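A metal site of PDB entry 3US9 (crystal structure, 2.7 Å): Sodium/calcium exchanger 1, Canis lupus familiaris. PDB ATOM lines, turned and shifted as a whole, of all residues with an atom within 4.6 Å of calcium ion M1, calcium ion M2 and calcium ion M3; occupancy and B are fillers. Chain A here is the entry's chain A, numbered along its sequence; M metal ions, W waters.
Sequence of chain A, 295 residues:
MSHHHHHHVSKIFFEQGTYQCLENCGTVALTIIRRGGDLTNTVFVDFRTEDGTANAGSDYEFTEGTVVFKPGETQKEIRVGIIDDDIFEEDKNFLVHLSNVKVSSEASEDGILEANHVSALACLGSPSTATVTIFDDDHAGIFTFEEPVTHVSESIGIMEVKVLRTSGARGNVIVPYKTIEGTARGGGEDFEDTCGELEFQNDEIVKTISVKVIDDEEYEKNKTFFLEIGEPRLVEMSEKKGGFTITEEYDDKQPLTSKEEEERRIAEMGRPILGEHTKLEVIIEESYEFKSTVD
OD1 of Asp 84 lies close to OE1 of Glu 23 (2.6 Å).
N of Ile 83 lies within hydrogen-bond range of O of Asp 59, 3.5 Å away.
Within 4 Å of calcium ion M1: Glu 23, Asp 84, Asp 85, Asp 137 and Asp 138.
The nearest printed residue that does not touch calcium ion M1 is Asp 136 (4.4 Å).
Six residues have an atom within 4 Å of calcium ion M2: Glu 23, Asp 85, Ile 87, Glu 89, Asp 136 and Asp 138.
Asp 59 touches calcium ion M3.
Along chain A the residues within 4 Å of calcium ion M3 span positions 23 to 89.
Calcium ion M1 is bound by the side-chain carboxylate (OD2) of Asp 138 (2.2 Å), the side-chain carboxylate (OD2) of Asp 137 (2.3 Å), the side-chain carboxylate (OD1) of Asp 84 (2.4 Å), the backbone carbonyl oxygen (O) of Asp 85 (2.5 Å) and the side-chain carboxylate (OD1) of Asp 138 (2.7 Å).
Slightly farther from calcium ion M1 lies OE1 of Glu 23 (3.0 Å).
Calcium ion M2 is bound by OD1 of Asp 138 (1.9 Å), OE2 of Glu 89 (2.5 Å), OD1 of Asp 136 (2.6 Å), O of Ile 87 (2.7 Å), OE2 of Glu 23 (2.7 Å) and OD1 of Asp 85 (2.8 Å).
Slightly farther from calcium ion M2 lies OE1 of Glu 23 (3.1 Å).
Calcium ion M3 is bound by OE2 of Glu 89, 2.6 Å away.
OE2 of Glu 23 binds calcium ion M3, 2.8 Å away.
Slightly farther from calcium ion M3 lies OE1 of Glu 89 (2.9 Å).
Slightly farther from calcium ion M3 lies water W1 (3.0 Å).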
ATOM      1  N   GLU A  23      13.165 -10.031   2.784  1.00  0.00           N
ATOM      2  CA  GLU A  23      11.713  -9.940   2.746  1.00  0.00           C
ATOM      3  C   GLU A  23      11.214  -8.522   2.995  1.00  0.00           C
ATOM      4  O   GLU A  23      10.163  -8.130   2.484  1.00  0.00           O
ATOM      5  CB  GLU A  23      11.086 -10.896   3.757  1.00  0.00           C
ATOM      6  CG  GLU A  23       9.595 -11.044   3.572  1.00  0.00           C
ATOM      7  CD  GLU A  23       8.959 -11.855   4.677  1.00  0.00           C
ATOM      8  OE1 GLU A  23       8.005 -11.354   5.317  1.00  0.00           O
ATOM      9  OE2 GLU A  23       9.410 -12.996   4.890  1.00  0.00           O
ATOM     10  N   ASP A  59       4.178 -14.185  -0.721  1.00  0.00           N
ATOM     11  CA  ASP A  59       5.623 -13.983  -0.645  1.00  0.00           C
ATOM     12  C   ASP A  59       6.067 -12.785  -1.456  1.00  0.00           C
ATOM     13  O   ASP A  59       7.123 -12.210  -1.201  1.00  0.00           O
ATOM     14  CB  ASP A  59       6.367 -15.244  -1.102  1.00  0.00           C
ATOM     15  CG  ASP A  59       6.046 -16.461  -0.253  1.00  0.00           C
ATOM     16  OD1 ASP A  59       6.679 -16.611   0.809  1.00  0.00           O
ATOM     17  OD2 ASP A  59       5.169 -17.248  -0.653  1.00  0.00           O
ATOM     18  N   ILE A  83       6.405  -8.892  -0.547  1.00  0.00           N
ATOM     19  CA  ILE A  83       5.482  -8.846   0.585  1.00  0.00           C
ATOM     20  C   ILE A  83       6.147  -9.268   1.885  1.00  0.00           C
ATOM     21  O   ILE A  83       6.799 -10.311   1.962  1.00  0.00           O
ATOM     22  CB  ILE A  83       4.231  -9.708   0.346  1.00  0.00           C
ATOM     23  CG1 ILE A  83       3.453  -9.197  -0.873  1.00  0.00           C
ATOM     24  CG2 ILE A  83       3.342  -9.704   1.572  1.00  0.00           C
ATOM     25  CD1 ILE A  83       2.178  -9.949  -1.145  1.00  0.00           C
ATOM     26  N   ASP A  84       5.975  -8.443   2.905  1.00  0.00           N
ATOM     27  CA  ASP A  84       6.570  -8.702   4.197  1.00  0.00           C
ATOM     28  C   ASP A  84       5.529  -8.921   5.302  1.00  0.00           C
ATOM     29  O   ASP A  84       4.567  -8.158   5.422  1.00  0.00           O
ATOM     30  CB  ASP A  84       7.469  -7.528   4.582  1.00  0.00           C
ATOM     31  CG  ASP A  84       8.201  -7.757   5.875  1.00  0.00           C
ATOM     32  OD1 ASP A  84       8.270  -8.922   6.296  1.00  0.00           O
ATOM     33  OD2 ASP A  84       8.709  -6.773   6.453  1.00  0.00           O
ATOM     34  N   ASP A  85       5.741  -9.968   6.103  1.00  0.00           N
ATOM     35  CA  ASP A  85       4.954 -10.216   7.304  1.00  0.00           C
ATOM     36  C   ASP A  85       5.917 -10.594   8.436  1.00  0.00           C
ATOM     37  O   ASP A  85       7.111 -10.454   8.278  1.00  0.00           O
ATOM     38  CB  ASP A  85       3.912 -11.309   7.063  1.00  0.00           C
ATOM     39  CG  ASP A  85       4.517 -12.571   6.469  1.00  0.00           C
ATOM     40  OD1 ASP A  85       5.722 -12.800   6.650  1.00  0.00           O
ATOM     41  OD2 ASP A  85       3.772 -13.344   5.823  1.00  0.00           O
ATOM     42  N   ASP A  86       5.411 -11.067   9.566  1.00  0.00           N
ATOM     43  CA  ASP A  86       6.304 -11.362  10.686  1.00  0.00           C
ATOM     44  C   ASP A  86       6.495 -12.852  10.987  1.00  0.00           C
ATOM     45  O   ASP A  86       7.024 -13.222  12.035  1.00  0.00           O
ATOM     46  CB  ASP A  86       5.848 -10.625  11.954  1.00  0.00           C
ATOM     47  CG  ASP A  86       6.346  -9.193  12.005  1.00  0.00           C
ATOM     48  OD1 ASP A  86       6.838  -8.689  10.973  1.00  0.00           O
ATOM     49  OD2 ASP A  86       6.259  -8.568  13.090  1.00  0.00           O
ATOM     50  N   ILE A  87       6.073 -13.697  10.051  1.00  0.00           N
ATOM     51  CA  ILE A  87       6.089 -15.148  10.270  1.00  0.00           C
ATOM     52  C   ILE A  87       7.327 -15.825   9.684  1.00  0.00           C
ATOM     53  O   ILE A  87       7.446 -15.966   8.466  1.00  0.00           O
ATOM     54  CB  ILE A  87       4.846 -15.804   9.648  1.00  0.00           C
ATOM     55  CG1 ILE A  87       3.607 -14.928   9.859  1.00  0.00           C
ATOM     56  CG2 ILE A  87       4.639 -17.196  10.215  1.00  0.00           C
ATOM     57  CD1 ILE A  87       2.384 -15.415   9.103  1.00  0.00           C
ATOM     58  N   PHE A  88       8.239 -16.263  10.548  1.00  0.00           N
ATOM     59  CA  PHE A  88       9.473 -16.921  10.103  1.00  0.00           C
ATOM     60  C   PHE A  88       9.246 -17.942   8.985  1.00  0.00           C
ATOM     61  O   PHE A  88       8.386 -18.813   9.092  1.00  0.00           O
ATOM     62  CB  PHE A  88      10.171 -17.600  11.285  1.00  0.00           C
ATOM     63  CG  PHE A  88      11.457 -18.277  10.912  1.00  0.00           C
ATOM     64  CD1 PHE A  88      12.587 -17.537  10.602  1.00  0.00           C
ATOM     65  CD2 PHE A  88      11.546 -19.657  10.888  1.00  0.00           C
ATOM     66  CE1 PHE A  88      13.776 -18.161  10.260  1.00  0.00           C
ATOM     67  CE2 PHE A  88      12.735 -20.287  10.554  1.00  0.00           C
ATOM     68  CZ  PHE A  88      13.846 -19.543  10.237  1.00  0.00           C
ATOM     69  N   GLU A  89      10.039 -17.837   7.924  1.00  0.00           N
ATOM     70  CA  GLU A  89       9.962 -18.755   6.790  1.00  0.00           C
ATOM     71  C   GLU A  89      11.357 -19.172   6.330  1.00  0.00           C
ATOM     72  O   GLU A  89      12.341 -18.511   6.644  1.00  0.00           O
ATOM     73  CB  GLU A  89       9.255 -18.083   5.615  1.00  0.00           C
ATOM     74  CG  GLU A  89       7.942 -17.432   5.968  1.00  0.00           C
ATOM     75  CD  GLU A  89       7.541 -16.389   4.953  1.00  0.00           C
ATOM     76  OE1 GLU A  89       6.918 -16.741   3.931  1.00  0.00           O
ATOM     77  OE2 GLU A  89       7.867 -15.213   5.181  1.00  0.00           O
ATOM     78  N   ASP A 136      14.342 -14.629   4.350  1.00  0.00           N
ATOM     79  CA  ASP A 136      13.433 -14.199   5.397  1.00  0.00           C
ATOM     80  C   ASP A 136      14.130 -13.482   6.553  1.00  0.00           C
ATOM     81  O   ASP A 136      15.302 -13.776   6.843  1.00  0.00           O
ATOM     82  CB  ASP A 136      12.679 -15.396   5.942  1.00  0.00           C
ATOM     83  CG  ASP A 136      11.574 -15.002   6.895  1.00  0.00           C
ATOM     84  OD1 ASP A 136      10.545 -14.550   6.382  1.00  0.00           O
ATOM     85  OD2 ASP A 136      11.722 -15.155   8.141  1.00  0.00           O
ATOM     86  N   ASP A 137      13.436 -12.557   7.202  1.00  0.00           N
ATOM     87  CA  ASP A 137      14.043 -11.756   8.255  1.00  0.00           C
ATOM     88  C   ASP A 137      13.249 -11.787   9.547  1.00  0.00           C
ATOM     89  O   ASP A 137      13.169 -10.785  10.258  1.00  0.00           O
ATOM     90  CB  ASP A 137      14.211 -10.307   7.784  1.00  0.00           C
ATOM     91  CG  ASP A 137      12.887  -9.608   7.569  1.00  0.00           C
ATOM     92  OD1 ASP A 137      12.888  -8.374   7.422  1.00  0.00           O
ATOM     93  OD2 ASP A 137      11.844 -10.294   7.552  1.00  0.00           O
ATOM     94  N   ASP A 138      12.725 -12.957   9.889  1.00  0.00           N
ATOM     95  CA  ASP A 138      11.884 -13.091  11.079  1.00  0.00           C
ATOM     96  C   ASP A 138      12.379 -14.086  12.143  1.00  0.00           C
ATOM     97  O   ASP A 138      11.593 -14.475  13.010  1.00  0.00           O
ATOM     98  CB  ASP A 138      10.449 -13.434  10.668  1.00  0.00           C
ATOM     99  CG  ASP A 138       9.923 -12.523   9.572  1.00  0.00           C
ATOM    100  OD1 ASP A 138       9.381 -13.036   8.572  1.00  0.00           O
ATOM    101  OD2 ASP A 138      10.042 -11.290   9.724  1.00  0.00           O
HETATM  102 CA    CA M   1       9.544 -10.449   7.703  1.00  0.00          CA
HETATM  103 CA    CA M   2       8.254 -13.764   7.218  1.00  0.00          CA
HETATM  104 CA    CA M   3       8.013 -14.256   2.818  1.00  0.00          CA
HETATM  105  O   HOH W   1       5.273 -13.258   3.569  1.00  0.00           O
